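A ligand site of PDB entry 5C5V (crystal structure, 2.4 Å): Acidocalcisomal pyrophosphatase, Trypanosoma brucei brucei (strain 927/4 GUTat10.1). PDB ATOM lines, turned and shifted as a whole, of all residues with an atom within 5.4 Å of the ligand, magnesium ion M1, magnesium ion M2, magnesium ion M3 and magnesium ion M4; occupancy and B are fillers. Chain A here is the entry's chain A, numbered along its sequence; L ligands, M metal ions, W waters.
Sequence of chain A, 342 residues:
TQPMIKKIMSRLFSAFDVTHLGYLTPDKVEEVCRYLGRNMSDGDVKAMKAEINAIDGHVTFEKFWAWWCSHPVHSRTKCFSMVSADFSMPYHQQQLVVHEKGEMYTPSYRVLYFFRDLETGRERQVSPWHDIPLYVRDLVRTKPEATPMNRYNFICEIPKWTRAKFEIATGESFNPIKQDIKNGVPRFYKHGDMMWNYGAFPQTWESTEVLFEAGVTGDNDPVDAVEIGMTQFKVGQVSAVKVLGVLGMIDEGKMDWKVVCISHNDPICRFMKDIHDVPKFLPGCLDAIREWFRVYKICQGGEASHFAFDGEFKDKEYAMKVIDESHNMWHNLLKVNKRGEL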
ATOM      1  N   GLU A 157      31.558 -12.743  24.693  1.00  0.00           N
ATOM      2  CA  GLU A 157      32.009 -11.417  24.266  1.00  0.00           C
ATOM      3  C   GLU A 157      31.183 -10.334  24.980  1.00  0.00           C
ATOM      4  O   GLU A 157      31.714  -9.299  25.403  1.00  0.00           O
ATOM      5  CB  GLU A 157      31.877 -11.281  22.751  1.00  0.00           C
ATOM      6  CG  GLU A 157      32.737 -12.288  21.986  1.00  0.00           C
ATOM      7  CD  GLU A 157      32.411 -12.408  20.505  1.00  0.00           C
ATOM      8  OE1 GLU A 157      31.210 -12.318  20.132  1.00  0.00           O
ATOM      9  OE2 GLU A 157      33.364 -12.614  19.709  1.00  0.00           O
ATOM     10  N   LYS A 165      29.725  -3.571  22.752  1.00  0.00           N
ATOM     11  CA  LYS A 165      29.789  -4.626  21.742  1.00  0.00           C
ATOM     12  C   LYS A 165      31.218  -5.133  21.523  1.00  0.00           C
ATOM     13  O   LYS A 165      31.876  -4.785  20.548  1.00  0.00           O
ATOM     14  CB  LYS A 165      29.179  -4.133  20.435  1.00  0.00           C
ATOM     15  CG  LYS A 165      28.345  -5.179  19.698  1.00  0.00           C
ATOM     16  CD  LYS A 165      29.187  -6.266  19.067  1.00  0.00           C
ATOM     17  CE  LYS A 165      28.336  -7.283  18.302  1.00  0.00           C
ATOM     18  NZ  LYS A 165      29.156  -8.389  17.708  1.00  0.00           N
ATOM     19  N   GLU A 167      33.971  -8.033  20.622  1.00  0.00           N
ATOM     20  CA  GLU A 167      34.069  -8.991  19.523  1.00  0.00           C
ATOM     21  C   GLU A 167      35.486  -9.581  19.516  1.00  0.00           C
ATOM     22  O   GLU A 167      36.454  -8.880  19.797  1.00  0.00           O
ATOM     23  CB  GLU A 167      33.827  -8.334  18.168  1.00  0.00           C
ATOM     24  CG  GLU A 167      32.382  -8.126  17.766  1.00  0.00           C
ATOM     25  CD  GLU A 167      32.232  -7.555  16.348  1.00  0.00           C
ATOM     26  OE1 GLU A 167      33.274  -7.377  15.663  1.00  0.00           O
ATOM     27  OE2 GLU A 167      31.077  -7.287  15.928  1.00  0.00           O
ATOM     28  N   ASP A 180      34.108  -3.461  19.145  1.00  0.00           N
ATOM     29  CA  ASP A 180      33.816  -3.088  17.782  1.00  0.00           C
ATOM     30  C   ASP A 180      33.720  -1.556  17.664  1.00  0.00           C
ATOM     31  O   ASP A 180      33.382  -0.873  18.628  1.00  0.00           O
ATOM     32  CB  ASP A 180      32.516  -3.759  17.336  1.00  0.00           C
ATOM     33  CG  ASP A 180      32.281  -3.659  15.847  1.00  0.00           C
ATOM     34  OD1 ASP A 180      33.246  -3.351  15.110  1.00  0.00           O
ATOM     35  OD2 ASP A 180      31.129  -3.906  15.419  1.00  0.00           O
ATOM     36  N   ARG A 187      31.678   0.928  19.887  1.00  0.00           N
ATOM     37  CA  ARG A 187      30.259   0.649  19.666  1.00  0.00           C
ATOM     38  C   ARG A 187      29.504   0.163  20.906  1.00  0.00           C
ATOM     39  O   ARG A 187      29.908  -0.792  21.578  1.00  0.00           O
ATOM     40  CB  ARG A 187      30.108  -0.360  18.527  1.00  0.00           C
ATOM     41  CG  ARG A 187      28.717  -0.876  18.262  1.00  0.00           C
ATOM     42  CD  ARG A 187      28.755  -1.987  17.214  1.00  0.00           C
ATOM     43  NE  ARG A 187      27.444  -2.559  16.912  1.00  0.00           N
ATOM     44  CZ  ARG A 187      27.255  -3.730  16.306  1.00  0.00           C
ATOM     45  NH1 ARG A 187      28.286  -4.480  15.944  1.00  0.00           N
ATOM     46  NH2 ARG A 187      26.024  -4.157  16.068  1.00  0.00           N
ATOM     47  N   TYR A 189      25.398  -0.947  21.867  1.00  0.00           N
ATOM     48  CA  TYR A 189      24.061  -1.160  21.329  1.00  0.00           C
ATOM     49  C   TYR A 189      23.184   0.047  21.632  1.00  0.00           C
ATOM     50  O   TYR A 189      23.083   0.483  22.783  1.00  0.00           O
ATOM     51  CB  TYR A 189      23.411  -2.395  21.924  1.00  0.00           C
ATOM     52  CG  TYR A 189      23.975  -3.700  21.460  1.00  0.00           C
ATOM     53  CD1 TYR A 189      24.273  -3.917  20.118  1.00  0.00           C
ATOM     54  CD2 TYR A 189      24.161  -4.735  22.352  1.00  0.00           C
ATOM     55  CE1 TYR A 189      24.766  -5.122  19.704  1.00  0.00           C
ATOM     56  CE2 TYR A 189      24.657  -5.949  21.949  1.00  0.00           C
ATOM     57  CZ  TYR A 189      24.953  -6.130  20.627  1.00  0.00           C
ATOM     58  OH  TYR A 189      25.438  -7.355  20.209  1.00  0.00           O
ATOM     59  N   TYR A 198      26.128 -13.194  25.315  1.00  0.00           N
ATOM     60  CA  TYR A 198      26.314 -13.270  23.892  1.00  0.00           C
ATOM     61  C   TYR A 198      27.791 -13.438  23.550  1.00  0.00           C
ATOM     62  O   TYR A 198      28.650 -12.868  24.204  1.00  0.00           O
ATOM     63  CB  TYR A 198      25.759 -12.009  23.233  1.00  0.00           C
ATOM     64  CG  TYR A 198      25.853 -12.000  21.736  1.00  0.00           C
ATOM     65  CD1 TYR A 198      24.910 -12.666  20.956  1.00  0.00           C
ATOM     66  CD2 TYR A 198      26.893 -11.352  21.089  1.00  0.00           C
ATOM     67  CE1 TYR A 198      25.001 -12.671  19.576  1.00  0.00           C
ATOM     68  CE2 TYR A 198      26.992 -11.359  19.705  1.00  0.00           C
ATOM     69  CZ  TYR A 198      26.040 -12.004  18.962  1.00  0.00           C
ATOM     70  OH  TYR A 198      26.136 -12.008  17.592  1.00  0.00           O
ATOM     71  N   GLY A 199      28.086 -14.240  22.532  1.00  0.00           N
ATOM     72  CA  GLY A 199      29.463 -14.470  22.148  1.00  0.00           C
ATOM     73  C   GLY A 199      29.602 -15.341  20.914  1.00  0.00           C
ATOM     74  O   GLY A 199      28.832 -15.223  19.969  1.00  0.00           O
ATOM     75  N   ALA A 200      30.579 -16.243  20.933  1.00  0.00           N
ATOM     76  CA  ALA A 200      30.883 -17.020  19.757  1.00  0.00           C
ATOM     77  C   ALA A 200      31.452 -18.389  20.101  1.00  0.00           C
ATOM     78  O   ALA A 200      31.899 -18.629  21.226  1.00  0.00           O
ATOM     79  CB  ALA A 200      31.847 -16.256  18.863  1.00  0.00           C
ATOM     80  N   ASP A 219      28.678 -14.292   7.365  1.00  0.00           N
ATOM     81  CA  ASP A 219      29.035 -12.932   7.765  1.00  0.00           C
ATOM     82  C   ASP A 219      30.513 -12.809   8.133  1.00  0.00           C
ATOM     83  O   ASP A 219      30.930 -11.815   8.726  1.00  0.00           O
ATOM     84  CB  ASP A 219      28.141 -12.442   8.931  1.00  0.00           C
ATOM     85  CG  ASP A 219      28.622 -12.935  10.308  1.00  0.00           C
ATOM     86  OD1 ASP A 219      28.337 -12.218  11.285  1.00  0.00           O
ATOM     87  OD2 ASP A 219      29.279 -14.012  10.408  1.00  0.00           O
ATOM     88  N   ASP A 221      32.499 -14.259  10.254  1.00  0.00           N
ATOM     89  CA  ASP A 221      32.809 -14.261  11.690  1.00  0.00           C
ATOM     90  C   ASP A 221      32.629 -15.649  12.274  1.00  0.00           C
ATOM     91  O   ASP A 221      31.985 -16.503  11.674  1.00  0.00           O
ATOM     92  CB  ASP A 221      31.919 -13.270  12.450  1.00  0.00           C
ATOM     93  CG  ASP A 221      32.569 -11.922  12.702  1.00  0.00           C
ATOM     94  OD1 ASP A 221      33.785 -11.877  12.993  1.00  0.00           O
ATOM     95  OD2 ASP A 221      31.876 -10.889  12.650  1.00  0.00           O
ATOM     96  N   PRO A 222      33.182 -15.885  13.467  1.00  0.00           N
ATOM     97  CA  PRO A 222      32.827 -17.126  14.164  1.00  0.00           C
ATOM     98  C   PRO A 222      31.307 -17.228  14.344  1.00  0.00           C
ATOM     99  O   PRO A 222      30.631 -16.199  14.375  1.00  0.00           O
ATOM    100  CB  PRO A 222      33.536 -16.990  15.514  1.00  0.00           C
ATOM    101  CG  PRO A 222      34.636 -16.053  15.258  1.00  0.00           C
ATOM    102  CD  PRO A 222      34.152 -15.090  14.240  1.00  0.00           C
ATOM    103  N   ASP A 224      27.800 -17.328  15.992  1.00  0.00           N
ATOM    104  CA  ASP A 224      27.298 -16.578  17.141  1.00  0.00           C
ATOM    105  C   ASP A 224      26.450 -17.446  18.053  1.00  0.00           C
ATOM    106  O   ASP A 224      25.693 -18.296  17.594  1.00  0.00           O
ATOM    107  CB  ASP A 224      26.499 -15.372  16.656  1.00  0.00           C
ATOM    108  CG  ASP A 224      27.347 -14.353  15.899  1.00  0.00           C
ATOM    109  OD1 ASP A 224      28.493 -14.093  16.329  1.00  0.00           O
ATOM    110  OD2 ASP A 224      26.872 -13.830  14.882  1.00  0.00           O
ATOM    111  N   MET A 249      19.179 -16.311  11.333  1.00  0.00           N
ATOM    112  CA  MET A 249      19.264 -14.896  11.050  1.00  0.00           C
ATOM    113  C   MET A 249      20.081 -14.593   9.798  1.00  0.00           C
ATOM    114  O   MET A 249      21.224 -15.072   9.664  1.00  0.00           O
ATOM    115  CB  MET A 249      19.876 -14.169  12.244  1.00  0.00           C
ATOM    116  CG  MET A 249      20.082 -12.679  12.035  1.00  0.00           C
ATOM    117  SD  MET A 249      20.723 -11.927  13.544  1.00  0.00           S
ATOM    118  CE  MET A 249      20.928 -10.218  13.011  1.00  0.00           C
ATOM    119  N   ASP A 251      21.726 -11.350   8.236  1.00  0.00           N
ATOM    120  CA  ASP A 251      22.082 -10.018   8.697  1.00  0.00           C
ATOM    121  C   ASP A 251      22.808  -9.231   7.598  1.00  0.00           C
ATOM    122  O   ASP A 251      23.925  -9.593   7.224  1.00  0.00           O
ATOM    123  CB  ASP A 251      22.957 -10.136   9.963  1.00  0.00           C
ATOM    124  CG  ASP A 251      23.263  -8.795  10.599  1.00  0.00           C
ATOM    125  OD1 ASP A 251      22.760  -7.769  10.099  1.00  0.00           O
ATOM    126  OD2 ASP A 251      24.009  -8.767  11.609  1.00  0.00           O
ATOM    127  N   GLU A 252      22.179  -8.172   7.083  1.00  0.00           N
ATOM    128  CA  GLU A 252      22.802  -7.379   6.006  1.00  0.00           C
ATOM    129  C   GLU A 252      23.238  -8.248   4.827  1.00  0.00           C
ATOM    130  O   GLU A 252      24.321  -8.069   4.269  1.00  0.00           O
ATOM    131  CB  GLU A 252      24.016  -6.593   6.554  1.00  0.00           C
ATOM    132  CG  GLU A 252      23.670  -5.533   7.604  1.00  0.00           C
ATOM    133  CD  GLU A 252      24.827  -5.241   8.586  1.00  0.00           C
ATOM    134  OE1 GLU A 252      25.831  -5.991   8.607  1.00  0.00           O
ATOM    135  OE2 GLU A 252      24.744  -4.260   9.353  1.00  0.00           O
ATOM    136  N   ASP A 256      23.930 -15.569   9.283  1.00  0.00           N
ATOM    137  CA  ASP A 256      24.374 -15.146  10.594  1.00  0.00           C
ATOM    138  C   ASP A 256      23.627 -15.924  11.669  1.00  0.00           C
ATOM    139  O   ASP A 256      22.964 -15.332  12.536  1.00  0.00           O
ATOM    140  CB  ASP A 256      24.171 -13.644  10.745  1.00  0.00           C
ATOM    141  CG  ASP A 256      25.086 -13.024  11.752  1.00  0.00           C
ATOM    142  OD1 ASP A 256      26.085 -13.686  12.143  1.00  0.00           O
ATOM    143  OD2 ASP A 256      24.828 -11.870  12.158  1.00  0.00           O
ATOM    144  N   LYS A 258      22.246 -17.831  14.751  1.00  0.00           N
ATOM    145  CA  LYS A 258      22.301 -17.521  16.174  1.00  0.00           C
ATOM    146  C   LYS A 258      21.953 -18.774  16.961  1.00  0.00           C
ATOM    147  O   LYS A 258      20.789 -19.163  17.037  1.00  0.00           O
ATOM    148  CB  LYS A 258      21.341 -16.382  16.519  1.00  0.00           C
ATOM    149  CG  LYS A 258      21.703 -15.043  15.887  1.00  0.00           C
ATOM    150  CD  LYS A 258      22.868 -14.386  16.604  1.00  0.00           C
ATOM    151  CE  LYS A 258      23.216 -13.045  15.967  1.00  0.00           C
ATOM    152  NZ  LYS A 258      23.801 -13.221  14.613  1.00  0.00           N
ATOM    153  N   TYR A 296      17.186  -4.760  16.226  1.00  0.00           N
ATOM    154  CA  TYR A 296      18.139  -3.959  17.008  1.00  0.00           C
ATOM    155  C   TYR A 296      18.949  -2.943  16.202  1.00  0.00           C
ATOM    156  O   TYR A 296      19.355  -1.938  16.744  1.00  0.00           O
ATOM    157  CB  TYR A 296      19.090  -4.872  17.810  1.00  0.00           C
ATOM    158  CG  TYR A 296      20.194  -5.604  17.051  1.00  0.00           C
ATOM    159  CD1 TYR A 296      21.532  -5.364  17.344  1.00  0.00           C
ATOM    160  CD2 TYR A 296      19.903  -6.564  16.086  1.00  0.00           C
ATOM    161  CE1 TYR A 296      22.568  -6.051  16.674  1.00  0.00           C
ATOM    162  CE2 TYR A 296      20.918  -7.241  15.392  1.00  0.00           C
ATOM    163  CZ  TYR A 296      22.248  -6.994  15.711  1.00  0.00           C
ATOM    164  OH  TYR A 296      23.239  -7.658  15.052  1.00  0.00           O
ATOM    165  N   LYS A 297      19.151  -3.180  14.916  1.00  0.00           N
ATOM    166  CA  LYS A 297      19.955  -2.244  14.124  1.00  0.00           C
ATOM    167  C   LYS A 297      19.131  -1.135  13.469  1.00  0.00           C
ATOM    168  O   LYS A 297      19.690  -0.184  12.924  1.00  0.00           O
ATOM    169  CB  LYS A 297      20.748  -2.996  13.044  1.00  0.00           C
ATOM    170  CG  LYS A 297      21.919  -3.823  13.601  1.00  0.00           C
ATOM    171  CD  LYS A 297      22.656  -4.583  12.484  1.00  0.00           C
ATOM    172  CE  LYS A 297      23.760  -5.487  13.053  1.00  0.00           C
ATOM    173  NZ  LYS A 297      24.557  -6.202  12.001  1.00  0.00           N
HETATM  174  P1  LIG L   1      26.690  -7.692  14.621  1.00  0.00           P
HETATM  175  O1  LIG L   1      27.970  -6.855  14.370  1.00  0.00           O
HETATM  176  O2  LIG L   1      26.147  -8.172  13.244  1.00  0.00           O
HETATM  177  O3  LIG L   1      25.675  -6.841  15.432  1.00  0.00           O
HETATM  178  N1  LIG L   1      27.073  -8.965  15.571  1.00  0.00           N
HETATM  179  P2  LIG L   1      27.970 -10.251  15.082  1.00  0.00           P
HETATM  180  O4  LIG L   1      29.337  -9.785  14.484  1.00  0.00           O
HETATM  181  O5  LIG L   1      27.177 -10.965  14.008  1.00  0.00           O
HETATM  182  O6  LIG L   1      28.214 -11.137  16.223  1.00  0.00           O
HETATM  183 MG    MG M   1      25.476 -10.078  12.737  1.00  0.00          MG
HETATM  184 MG    MG M   2      27.576 -12.867  13.258  1.00  0.00          MG
HETATM  185 MG    MG M   3      29.970  -7.562  14.023  1.00  0.00          MG
HETATM  186 MG    MG M   4      29.505 -12.463  15.868  1.00  0.00          MG
HETATM  187  O   HOH W   1      28.629 -14.782  12.908  1.00  0.00           O
HETATM  188  O   HOH W   2      31.972  -8.170  13.295  1.00  0.00           O
HETATM  189  O   HOH W   3      29.326 -12.294  13.825  1.00  0.00           O
HETATM  190  O   HOH W   4      29.361  -7.570  12.007  1.00  0.00           O
HETATM  191  O   HOH W   5      24.341 -10.084  14.484  1.00  0.00           O
HETATM  192  O   HOH W   6      26.895  -9.958  11.016  1.00  0.00           O
HETATM  193  O   HOH W   7      31.222 -11.016  16.107  1.00  0.00           O
HETATM  194  O   HOH W   8      31.224 -14.010  15.670  1.00  0.00           O
HETATM  195  O   HOH W   9      30.384  -5.706  13.277  1.00  0.00           O
HETATM  196  O   HOH W  10      29.906 -12.924  17.847  1.00  0.00           O
HETATM  197  O   HOH W  11      25.345  -8.591  17.700  1.00  0.00           O
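O6 of the ligand is bound to magnesium ion M4. Magnesium ion M4 is bound by OD1 of Asp 224 (2.0 Å). Water W3 binds magnesium ion M4, 2.1 Å away. Water W10 binds magnesium ion M4 (2.1 Å). Water W7 binds magnesium ion M4, at 2.3 Å. Magnesium ion M4 is bound by water W8 (2.3 Å).
Of the 20 residues printed, 3 come within 4 Å of magnesium ion M1.
Water W9 is bound to magnesium ion M3, at 2.0 Å. Water W4 is bound to magnesium ion M3 (2.1 Å). O1 of the ligand is bound to magnesium ion M3 (2.1 Å). Water W2 is bound to magnesium ion M3 (2.2 Å). OE2 of Glu 167 is bound to magnesium ion M3 (2.2 Å). An oxygen (O4) of the ligand is bound to magnesium ion M3 (2.4 Å). Magnesium ion M3 has six donor atoms within binding distance.
Magnesium ion M2 is bound by water W3 (1.9 Å), the side-chain carboxylate (OD2) of Asp 224 (2.0 Å), the side-chain carboxylate (OD1) of Asp 256 (2.0 Å), an oxygen (O5) of the ligand (2.1 Å), the side-chain carboxylate (OD1) of Asp 219 (2.2 Å) and water W1 (2.2 Å). Magnesium ion M2 has six donor atoms within binding distance.
Tyr 198 touches magnesium ion M4 (OH to MG, 3.8 Å). Of the 20 residues printed, 2 come within 4 Å of magnesium ion M4.
Of the 20 residues printed, 3 come within 4 Å of magnesium ion M2.
The side-chain hydroxyl (OH) of Tyr 296 sits at hydrogen-bond distance from an oxygen (O3) of the ligand (2.6 Å). The side-chain hydroxyl (OH) of Tyr 198 lies close to an oxygen (O6) of the ligand (2.6 Å). An oxygen (O3) of the ligand lies within salt-bridge range of the guanidinium group (NH2) of Arg 187. The side-chain amino group (NZ) of Lys 297 is in salt-bridge range of an oxygen (O3) of the ligand (3.7 Å). The side-chain amino group (NZ) of Lys 165 lies close to an oxygen (O6) of the ligand (3.3 Å).
OD2 of Asp 221 sits close to O4 of the ligand, at 3.3 Å. Hydrophobic or aromatic side chains within 4 Å of the ligand: Tyr 198 and Tyr 296.
OD2 of Asp 256 is bound to magnesium ion M1 (2.0 Å). Water W5 binds magnesium ion M1 (2.1 Å). An oxygen (O2) of the ligand binds magnesium ion M1, at 2.1 Å. Magnesium ion M1 is bound by water W6 (2.2 Å). Magnesium ion M1 is bound by OD2 of Asp 251 (2.3 Å). O5 of the ligand binds magnesium ion M1, at 2.3 Å. Magnesium ion M1 has six donor atoms within binding distance.
Merely in contact with magnesium ion M3: Lys 165.
O of Asp 256 is in hydrogen-bond range of NZ of Lys 258 (3.1 Å). The backbone NH (N) of Asp 256 lies within hydrogen-bond range of the backbone carbonyl oxygen (O) of Met 249 (2.8 Å). The backbone NH (N) of Asp 221 sits at hydrogen-bond distance from the side-chain carboxylate (OD2) of Asp 219, at 3.2 Å. The side-chain carboxylate of Glu 167 sits close to the guanidinium group of Arg 187. The side-chain carboxylate (OE2) of Glu 167 sits close to the side-chain amino group (NZ) of Lys 165 (2.8 Å). The side-chain carboxylate (OD1) of Asp 251 lies within salt-bridge range of the side-chain amino group (NZ) of Lys 297, 3.0 Å away. The backbone NH of Glu 157 sits at hydrogen-bond distance from the backbone carbonyl oxygen of Tyr 198 (3.0 Å). O of Lys 165 sits at hydrogen-bond distance from N of Asp 180, at 3.0 Å.
Water W5 lies within hydrogen-bond range of the side-chain hydroxyl (OH) of Tyr 296 (2.7 Å), a nitrogen (N1) of the ligand (3.1 Å) and the side-chain amino group (NZ) of Lys 258 (3.2 Å). Water W1 lies within hydrogen-bond range of the side-chain carboxylate of Asp 219 and the backbone carbonyl oxygen of Pro 222. Water W2 lies within hydrogen-bond range of the side-chain carboxylate (OD2) of Asp 221 (2.8 Å) and the side-chain carboxylate (OE1) of Glu 167 (2.8 Å). Water W10 bridges the side-chain carboxylate of Glu 157 and the backbone carbonyl oxygen of Gly 199. Water W11 lies within hydrogen-bond range of N1 of the ligand and OH of Tyr 189.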
